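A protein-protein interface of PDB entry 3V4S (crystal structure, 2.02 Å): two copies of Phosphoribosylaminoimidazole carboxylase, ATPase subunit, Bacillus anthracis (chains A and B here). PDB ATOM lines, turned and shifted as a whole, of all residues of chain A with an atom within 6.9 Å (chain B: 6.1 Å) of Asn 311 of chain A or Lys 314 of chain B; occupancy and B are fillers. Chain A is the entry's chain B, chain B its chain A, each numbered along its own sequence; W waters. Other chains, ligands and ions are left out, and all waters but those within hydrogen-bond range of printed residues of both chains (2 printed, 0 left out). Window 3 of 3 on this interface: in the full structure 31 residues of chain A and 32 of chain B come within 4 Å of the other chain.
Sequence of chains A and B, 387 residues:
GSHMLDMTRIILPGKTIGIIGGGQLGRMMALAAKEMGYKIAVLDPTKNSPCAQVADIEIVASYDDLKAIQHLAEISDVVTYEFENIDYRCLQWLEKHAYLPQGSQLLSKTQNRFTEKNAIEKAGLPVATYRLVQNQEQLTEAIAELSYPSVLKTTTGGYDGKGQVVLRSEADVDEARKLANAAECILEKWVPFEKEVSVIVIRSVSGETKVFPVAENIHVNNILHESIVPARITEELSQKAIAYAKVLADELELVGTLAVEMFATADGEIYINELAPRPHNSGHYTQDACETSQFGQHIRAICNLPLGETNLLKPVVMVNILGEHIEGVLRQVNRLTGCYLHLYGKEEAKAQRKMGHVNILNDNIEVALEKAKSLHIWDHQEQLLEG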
ATOM      1  N   VAL A 211      37.028   8.738   0.275  1.00  0.00           N
ATOM      2  CA  VAL A 211      36.966   7.358  -0.140  1.00  0.00           C
ATOM      3  C   VAL A 211      35.925   7.236  -1.247  1.00  0.00           C
ATOM      4  O   VAL A 211      34.831   7.793  -1.136  1.00  0.00           O
ATOM      5  CB  VAL A 211      36.587   6.448   1.041  1.00  0.00           C
ATOM      6  CG1 VAL A 211      36.569   5.006   0.601  1.00  0.00           C
ATOM      7  CG2 VAL A 211      37.552   6.634   2.215  1.00  0.00           C
ATOM      8  N   PHE A 212      36.263   6.507  -2.306  1.00  0.00           N
ATOM      9  CA  PHE A 212      35.304   6.207  -3.371  1.00  0.00           C
ATOM     10  C   PHE A 212      34.351   5.089  -2.994  1.00  0.00           C
ATOM     11  O   PHE A 212      34.626   4.329  -2.061  1.00  0.00           O
ATOM     12  CB  PHE A 212      36.031   5.874  -4.675  1.00  0.00           C
ATOM     13  CG  PHE A 212      36.592   7.083  -5.366  1.00  0.00           C
ATOM     14  CD1 PHE A 212      37.927   7.442  -5.201  1.00  0.00           C
ATOM     15  CD2 PHE A 212      35.774   7.886  -6.163  1.00  0.00           C
ATOM     16  CE1 PHE A 212      38.441   8.571  -5.822  1.00  0.00           C
ATOM     17  CE2 PHE A 212      36.289   9.014  -6.797  1.00  0.00           C
ATOM     18  CZ  PHE A 212      37.621   9.352  -6.633  1.00  0.00           C
ATOM     19  N   PRO A 213      33.226   4.974  -3.720  1.00  0.00           N
ATOM     20  CA  PRO A 213      32.308   3.855  -3.488  1.00  0.00           C
ATOM     21  C   PRO A 213      32.959   2.481  -3.720  1.00  0.00           C
ATOM     22  O   PRO A 213      33.851   2.331  -4.567  1.00  0.00           O
ATOM     23  CB  PRO A 213      31.194   4.094  -4.508  1.00  0.00           C
ATOM     24  CG  PRO A 213      31.208   5.560  -4.737  1.00  0.00           C
ATOM     25  CD  PRO A 213      32.661   5.971  -4.647  1.00  0.00           C
ATOM     26  N   ALA A 289      31.357   8.148 -13.624  1.00  0.00           N
ATOM     27  CA  ALA A 289      30.250   7.889 -12.674  1.00  0.00           C
ATOM     28  C   ALA A 289      30.342   8.656 -11.353  1.00  0.00           C
ATOM     29  O   ALA A 289      29.359   8.733 -10.600  1.00  0.00           O
ATOM     30  CB  ALA A 289      30.092   6.399 -12.408  1.00  0.00           C
ATOM     31  N   CYS A 290      31.494   9.248 -11.081  1.00  0.00           N
ATOM     32  CA  CYS A 290      31.647  10.010  -9.839  1.00  0.00           C
ATOM     33  C   CYS A 290      31.778  11.481 -10.073  1.00  0.00           C
ATOM     34  O   CYS A 290      32.094  11.927 -11.177  1.00  0.00           O
ATOM     35  CB  CYS A 290      32.841   9.513  -9.011  1.00  0.00           C
ATOM     36  SG  CYS A 290      32.574   7.870  -8.352  1.00  0.00           S
ATOM     37  N   GLU A 291      31.573  12.235  -9.005  1.00  0.00           N
ATOM     38  CA  GLU A 291      31.697  13.674  -9.056  1.00  0.00           C
ATOM     39  C   GLU A 291      33.153  14.092  -9.384  1.00  0.00           C
ATOM     40  O   GLU A 291      33.381  15.071 -10.110  1.00  0.00           O
ATOM     41  CB  GLU A 291      31.175  14.249  -7.726  1.00  0.00           C
ATOM     42  CG  GLU A 291      30.887  15.737  -7.742  1.00  0.00           C
ATOM     43  CD  GLU A 291      30.220  16.220  -6.464  1.00  0.00           C
ATOM     44  OE1 GLU A 291      30.602  17.317  -5.961  1.00  0.00           O
ATOM     45  OE2 GLU A 291      29.305  15.504  -5.974  1.00  0.00           O
ATOM     46  N   THR A 292      34.123  13.318  -8.885  1.00  0.00           N
ATOM     47  CA  THR A 292      35.553  13.490  -9.208  1.00  0.00           C
ATOM     48  C   THR A 292      36.143  12.133  -9.623  1.00  0.00           C
ATOM     49  O   THR A 292      35.770  11.093  -9.071  1.00  0.00           O
ATOM     50  CB  THR A 292      36.374  13.992  -7.994  1.00  0.00           C
ATOM     51  OG1 THR A 292      35.625  14.967  -7.256  1.00  0.00           O
ATOM     52  CG2 THR A 292      37.708  14.593  -8.434  1.00  0.00           C
ATOM     53  N   GLY A 308      37.970  16.748  -4.302  1.00  0.00           N
ATOM     54  CA  GLY A 308      36.624  16.800  -4.851  1.00  0.00           C
ATOM     55  C   GLY A 308      35.749  15.795  -4.135  1.00  0.00           C
ATOM     56  O   GLY A 308      36.242  14.978  -3.360  1.00  0.00           O
ATOM     57  N   GLU A 309      34.447  15.840  -4.387  1.00  0.00           N
ATOM     58  CA  GLU A 309      33.537  14.855  -3.802  1.00  0.00           C
ATOM     59  C   GLU A 309      33.602  13.549  -4.593  1.00  0.00           C
ATOM     60  O   GLU A 309      33.978  13.548  -5.781  1.00  0.00           O
ATOM     61  CB  GLU A 309      32.105  15.399  -3.714  1.00  0.00           C
ATOM     62  CG  GLU A 309      32.004  16.775  -3.044  1.00  0.00           C
ATOM     63  CD  GLU A 309      32.609  16.811  -1.630  1.00  0.00           C
ATOM     64  OE1 GLU A 309      32.445  15.841  -0.877  1.00  0.00           O
ATOM     65  OE2 GLU A 309      33.251  17.807  -1.259  1.00  0.00           O
ATOM     66  N   THR A 310      33.228  12.452  -3.934  1.00  0.00           N
ATOM     67  CA  THR A 310      33.347  11.111  -4.500  1.00  0.00           C
ATOM     68  C   THR A 310      31.992  10.440  -4.653  1.00  0.00           C
ATOM     69  O   THR A 310      31.921   9.232  -4.888  1.00  0.00           O
ATOM     70  CB  THR A 310      34.233  10.187  -3.621  1.00  0.00           C
ATOM     71  OG1 THR A 310      33.663  10.099  -2.303  1.00  0.00           O
ATOM     72  CG2 THR A 310      35.661  10.708  -3.527  1.00  0.00           C
ATOM     73  N   ASN A 311      30.917  11.212  -4.526  1.00  0.00           N
ATOM     74  CA  ASN A 311      29.563  10.676  -4.722  1.00  0.00           C
ATOM     75  C   ASN A 311      29.433   9.904  -6.023  1.00  0.00           C
ATOM     76  O   ASN A 311      29.938  10.349  -7.065  1.00  0.00           O
ATOM     77  CB  ASN A 311      28.535  11.810  -4.713  1.00  0.00           C
ATOM     78  CG  ASN A 311      28.601  12.620  -3.449  1.00  0.00           C
ATOM     79  OD1 ASN A 311      28.330  12.105  -2.374  1.00  0.00           O
ATOM     80  ND2 ASN A 311      28.994  13.876  -3.562  1.00  0.00           N
ATOM     81  N   LEU A 312      28.769   8.755  -5.958  1.00  0.00           N
ATOM     82  CA  LEU A 312      28.399   8.032  -7.143  1.00  0.00           C
ATOM     83  C   LEU A 312      27.181   8.711  -7.774  1.00  0.00           C
ATOM     84  O   LEU A 312      26.096   8.694  -7.210  1.00  0.00           O
ATOM     85  CB  LEU A 312      28.067   6.581  -6.817  1.00  0.00           C
ATOM     86  CG  LEU A 312      27.814   5.703  -8.039  1.00  0.00           C
ATOM     87  CD1 LEU A 312      29.117   5.372  -8.765  1.00  0.00           C
ATOM     88  CD2 LEU A 312      27.094   4.430  -7.641  1.00  0.00           C
ATOM     89  N   LEU A 313      27.354   9.277  -8.956  1.00  0.00           N
ATOM     90  CA  LEU A 313      26.268  10.018  -9.595  1.00  0.00           C
ATOM     91  C   LEU A 313      25.349   9.170 -10.454  1.00  0.00           C
ATOM     92  O   LEU A 313      24.259   9.617 -10.797  1.00  0.00           O
ATOM     93  CB  LEU A 313      26.819  11.198 -10.400  1.00  0.00           C
ATOM     94  CG  LEU A 313      27.591  12.251  -9.596  1.00  0.00           C
ATOM     95  CD1 LEU A 313      28.176  13.296 -10.537  1.00  0.00           C
ATOM     96  CD2 LEU A 313      26.722  12.913  -8.531  1.00  0.00           C
ATOM     97  N   LYS A 314      25.796   7.968 -10.816  1.00  0.00           N
ATOM     98  CA  LYS A 314      25.005   7.036 -11.610  1.00  0.00           C
ATOM     99  C   LYS A 314      25.673   5.656 -11.518  1.00  0.00           C
ATOM    100  O   LYS A 314      26.909   5.579 -11.480  1.00  0.00           O
ATOM    101  CB  LYS A 314      24.902   7.528 -13.070  1.00  0.00           C
ATOM    102  CG  LYS A 314      23.999   6.705 -13.992  1.00  0.00           C
ATOM    103  CD  LYS A 314      23.377   7.565 -15.105  1.00  0.00           C
ATOM    104  CE  LYS A 314      22.424   6.741 -15.964  1.00  0.00           C
ATOM    105  NZ  LYS A 314      21.931   7.483 -17.156  1.00  0.00           N
ATOM    106  N   VAL B 229      22.221  25.866 -13.543  1.00  0.00           N
ATOM    107  CA  VAL B 229      21.512  24.702 -14.062  1.00  0.00           C
ATOM    108  C   VAL B 229      21.087  23.797 -12.905  1.00  0.00           C
ATOM    109  O   VAL B 229      21.946  23.381 -12.106  1.00  0.00           O
ATOM    110  CB  VAL B 229      22.402  23.877 -15.035  1.00  0.00           C
ATOM    111  CG1 VAL B 229      21.556  22.858 -15.779  1.00  0.00           C
ATOM    112  CG2 VAL B 229      23.118  24.791 -16.020  1.00  0.00           C
ATOM    113  N   PRO B 230      19.780  23.481 -12.803  1.00  0.00           N
ATOM    114  CA  PRO B 230      18.679  23.851 -13.707  1.00  0.00           C
ATOM    115  C   PRO B 230      18.366  25.344 -13.659  1.00  0.00           C
ATOM    116  O   PRO B 230      18.505  25.978 -12.602  1.00  0.00           O
ATOM    117  CB  PRO B 230      17.484  23.043 -13.171  1.00  0.00           C
ATOM    118  CG  PRO B 230      18.063  22.029 -12.221  1.00  0.00           C
ATOM    119  CD  PRO B 230      19.278  22.706 -11.652  1.00  0.00           C
ATOM    120  N   ASP B 288      31.280  18.829 -15.704  1.00  0.00           N
ATOM    121  CA  ASP B 288      31.257  18.244 -14.360  1.00  0.00           C
ATOM    122  C   ASP B 288      29.878  17.801 -13.906  1.00  0.00           C
ATOM    123  O   ASP B 288      29.766  16.985 -12.982  1.00  0.00           O
ATOM    124  CB  ASP B 288      31.863  19.230 -13.368  1.00  0.00           C
ATOM    125  CG  ASP B 288      33.333  19.454 -13.636  1.00  0.00           C
ATOM    126  OD1 ASP B 288      34.110  18.467 -13.547  1.00  0.00           O
ATOM    127  OD2 ASP B 288      33.702  20.597 -13.964  1.00  0.00           O
ATOM    128  N   ALA B 289      28.835  18.308 -14.558  1.00  0.00           N
ATOM    129  CA  ALA B 289      27.460  18.099 -14.044  1.00  0.00           C
ATOM    130  C   ALA B 289      26.581  17.166 -14.853  1.00  0.00           C
ATOM    131  O   ALA B 289      25.481  16.812 -14.408  1.00  0.00           O
ATOM    132  CB  ALA B 289      26.749  19.436 -13.834  1.00  0.00           C
ATOM    133  N   CYS B 290      27.045  16.778 -16.038  1.00  0.00           N
ATOM    134  CA  CYS B 290      26.239  15.952 -16.930  1.00  0.00           C
ATOM    135  C   CYS B 290      26.956  14.661 -17.202  1.00  0.00           C
ATOM    136  O   CYS B 290      28.181  14.561 -17.052  1.00  0.00           O
ATOM    137  CB  CYS B 290      25.970  16.661 -18.274  1.00  0.00           C
ATOM    138  SG  CYS B 290      24.840  18.053 -18.137  1.00  0.00           S
ATOM    139  N   ASN B 311      21.871  13.747 -19.276  1.00  0.00           N
ATOM    140  CA  ASN B 311      21.295  13.891 -17.934  1.00  0.00           C
ATOM    141  C   ASN B 311      22.079  14.827 -17.035  1.00  0.00           C
ATOM    142  O   ASN B 311      23.295  14.715 -16.946  1.00  0.00           O
ATOM    143  CB  ASN B 311      21.209  12.519 -17.264  1.00  0.00           C
ATOM    144  CG  ASN B 311      20.291  11.579 -18.017  1.00  0.00           C
ATOM    145  OD1 ASN B 311      19.121  11.892 -18.235  1.00  0.00           O
ATOM    146  ND2 ASN B 311      20.815  10.454 -18.445  1.00  0.00           N
ATOM    147  N   LEU B 312      21.373  15.741 -16.363  1.00  0.00           N
ATOM    148  CA  LEU B 312      21.962  16.527 -15.288  1.00  0.00           C
ATOM    149  C   LEU B 312      22.106  15.602 -14.099  1.00  0.00           C
ATOM    150  O   LEU B 312      21.109  15.058 -13.610  1.00  0.00           O
ATOM    151  CB  LEU B 312      21.080  17.717 -14.895  1.00  0.00           C
ATOM    152  CG  LEU B 312      21.734  18.667 -13.879  1.00  0.00           C
ATOM    153  CD1 LEU B 312      22.891  19.431 -14.504  1.00  0.00           C
ATOM    154  CD2 LEU B 312      20.724  19.634 -13.307  1.00  0.00           C
ATOM    155  N   LEU B 313      23.342  15.434 -13.636  1.00  0.00           N
ATOM    156  CA  LEU B 313      23.643  14.501 -12.564  1.00  0.00           C
ATOM    157  C   LEU B 313      23.750  15.203 -11.230  1.00  0.00           C
ATOM    158  O   LEU B 313      23.719  14.557 -10.192  1.00  0.00           O
ATOM    159  CB  LEU B 313      24.940  13.726 -12.866  1.00  0.00           C
ATOM    160  CG  LEU B 313      24.897  12.774 -14.066  1.00  0.00           C
ATOM    161  CD1 LEU B 313      26.155  11.921 -14.086  1.00  0.00           C
ATOM    162  CD2 LEU B 313      23.647  11.892 -14.064  1.00  0.00           C
ATOM    163  N   LYS B 314      23.880  16.522 -11.265  1.00  0.00           N
ATOM    164  CA  LYS B 314      23.964  17.335 -10.061  1.00  0.00           C
ATOM    165  C   LYS B 314      23.775  18.797 -10.462  1.00  0.00           C
ATOM    166  O   LYS B 314      24.317  19.215 -11.492  1.00  0.00           O
ATOM    167  CB  LYS B 314      25.334  17.149  -9.374  1.00  0.00           C
ATOM    168  CG  LYS B 314      25.406  17.777  -7.980  1.00  0.00           C
ATOM    169  CD  LYS B 314      26.142  16.894  -6.973  1.00  0.00           C
ATOM    170  CE  LYS B 314      26.569  17.704  -5.753  1.00  0.00           C
ATOM    171  NZ  LYS B 314      27.266  16.870  -4.732  1.00  0.00           N
ATOM    172  N   PRO B 315      23.035  19.585  -9.650  1.00  0.00           N
ATOM    173  CA  PRO B 315      22.901  21.013  -9.958  1.00  0.00           C
ATOM    174  C   PRO B 315      24.232  21.747  -9.920  1.00  0.00           C
ATOM    175  O   PRO B 315      25.129  21.365  -9.163  1.00  0.00           O
ATOM    176  CB  PRO B 315      21.959  21.507  -8.853  1.00  0.00           C
ATOM    177  CG  PRO B 315      21.075  20.308  -8.618  1.00  0.00           C
ATOM    178  CD  PRO B 315      22.098  19.193  -8.574  1.00  0.00           C
ATOM    179  N   VAL B 316      24.355  22.798 -10.722  1.00  0.00           N
ATOM    180  CA  VAL B 316      25.644  23.436 -10.896  1.00  0.00           C
ATOM    181  C   VAL B 316      25.538  24.934 -11.155  1.00  0.00           C
ATOM    182  O   VAL B 316      24.587  25.419 -11.785  1.00  0.00           O
ATOM    183  CB  VAL B 316      26.443  22.725 -12.036  1.00  0.00           C
ATOM    184  CG1 VAL B 316      25.598  22.634 -13.309  1.00  0.00           C
ATOM    185  CG2 VAL B 316      27.784  23.410 -12.299  1.00  0.00           C
ATOM    186  N   LEU B 361      29.357  22.535  -7.839  1.00  0.00           N
ATOM    187  CA  LEU B 361      28.328  21.511  -7.758  1.00  0.00           C
ATOM    188  C   LEU B 361      27.734  21.493  -6.347  1.00  0.00           C
ATOM    189  O   LEU B 361      28.449  21.646  -5.357  1.00  0.00           O
ATOM    190  CB  LEU B 361      28.893  20.129  -8.107  1.00  0.00           C
ATOM    191  CG  LEU B 361      29.402  19.825  -9.533  1.00  0.00           C
ATOM    192  CD1 LEU B 361      29.697  18.342  -9.697  1.00  0.00           C
ATOM    193  CD2 LEU B 361      28.437  20.240 -10.621  1.00  0.00           C
ATOM    194  N   ASN B 362      26.419  21.337  -6.272  1.00  0.00           N
ATOM    195  CA  ASN B 362      25.713  21.278  -4.996  1.00  0.00           C
ATOM    196  C   ASN B 362      24.310  20.795  -5.231  1.00  0.00           C
ATOM    197  O   ASN B 362      23.703  21.174  -6.218  1.00  0.00           O
ATOM    198  CB  ASN B 362      25.665  22.636  -4.299  1.00  0.00           C
ATOM    199  CG  ASN B 362      25.349  22.502  -2.811  1.00  0.00           C
ATOM    200  OD1 ASN B 362      24.209  22.236  -2.423  1.00  0.00           O
ATOM    201  ND2 ASN B 362      26.365  22.661  -1.980  1.00  0.00           N
ATOM    202  N   ASP B 363      23.800  19.957  -4.332  1.00  0.00           N
ATOM    203  CA  ASP B 363      22.405  19.519  -4.402  1.00  0.00           C
ATOM    204  C   ASP B 363      21.453  20.726  -4.417  1.00  0.00           C
ATOM    205  O   ASP B 363      20.361  20.644  -4.966  1.00  0.00           O
ATOM    206  CB  ASP B 363      22.061  18.616  -3.208  1.00  0.00           C
ATOM    207  CG  ASP B 363      22.820  17.295  -3.221  1.00  0.00           C
ATOM    208  OD1 ASP B 363      23.196  16.829  -2.131  1.00  0.00           O
ATOM    209  OD2 ASP B 363      23.040  16.719  -4.305  1.00  0.00           O
HETATM  210  O   HOH W   1      23.032  12.022  -9.776  1.00  0.00           O
HETATM  211  O   HOH W   2      35.169  16.390 -11.697  1.00  0.00           O
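Glu 291 of chain A touches Leu 361 of chain B.
ND2 of Asn 311 of chain A touches NZ of Lys 314 of chain B (3.6 Å).
O of Leu 313 of chain B touches CD2 of Leu 313 of chain A (3.8 Å).
The backbone NH (N) of Leu 313 of chain B is in hydrogen-bond range of the backbone carbonyl oxygen (O) of Ala 289 of chain B (2.7 Å).
ND2 of Asn 311 of chain A is in hydrogen-bond range of OE2 of Glu 291 of chain A, at 2.9 Å.
O of Ala 289 of chain A sits at hydrogen-bond distance from N of Leu 313 of chain A, 2.6 Å away.
Water W1 lies within hydrogen-bond range of O of Leu 313 of chain B and O of Leu 313 of chain A.
Water W2 bridges O of Glu 291 of chain A (2.7 Å) and OD1 of Asp 288 of chain B (3.0 Å).
Asn 311 of chain A touches Lys 314 of chain B, and with the chains exchanged Lys 314 of chain A touches Asn 311 of chain B.
Leu 313 of chain B touches its own counterpart, Leu 313 of chain A.
6 positions are printed for both chains.
Of the 5 pairs that touch across the chains among the printed residues, 3 have their exchanged pair printed and touching as well.
Ala 289 of chain A touches none of the printed residues of chain B.
Asn 311 of chain A touches just one residue of chain B: Lys 314.
Printed residues of chain B within 4 Å of Leu 313 of chain A: Leu 313 (3.8 Å).
Of the printed residues of chain B, Lys 314 of chain A touches Asn 311 (3.4 Å).
Of chain A, only Glu 291 and Asn 311 come within 4 Å of Lys 314 of chain B.
Printed residues of chain A within 4 Å of Leu 361 of chain B: Glu 291 (3.5 Å).
The nearest residue of chain A that does not touch Lys 314 of chain B is Leu 313 of chain A (4.3 Å).
The nearest printed residue of chain A that does not touch Asn 311 of chain B is Leu 313 of chain A (7.7 Å).
Of the 14 printed residues of chain B, 4 touch a printed residue of chain A.
Hydrophobic or aromatic side chains of chain B within 4 Å of the printed part of chain A: Leu 313 and Leu 361.
Hydrophobic or aromatic side chains of chain A within 4 Å of the printed part of chain B: Leu 313.
Among the printed residues, Asp or Glu carboxylates within 4 Å of a Lys or Arg side-chain nitrogen of the other chain: Glu 291 of chain A with Lys 314 of chain B.
The side-chain amino group (NZ) of Lys 314 of chain A lies close to the side-chain amide nitrogen (ND2) of Asn 311 of chain B (3.4 Å).
The side-chain amino group of Lys 314 of chain B is in salt-bridge range of the side-chain carboxylate of Glu 291 of chain A (2.8 Å).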
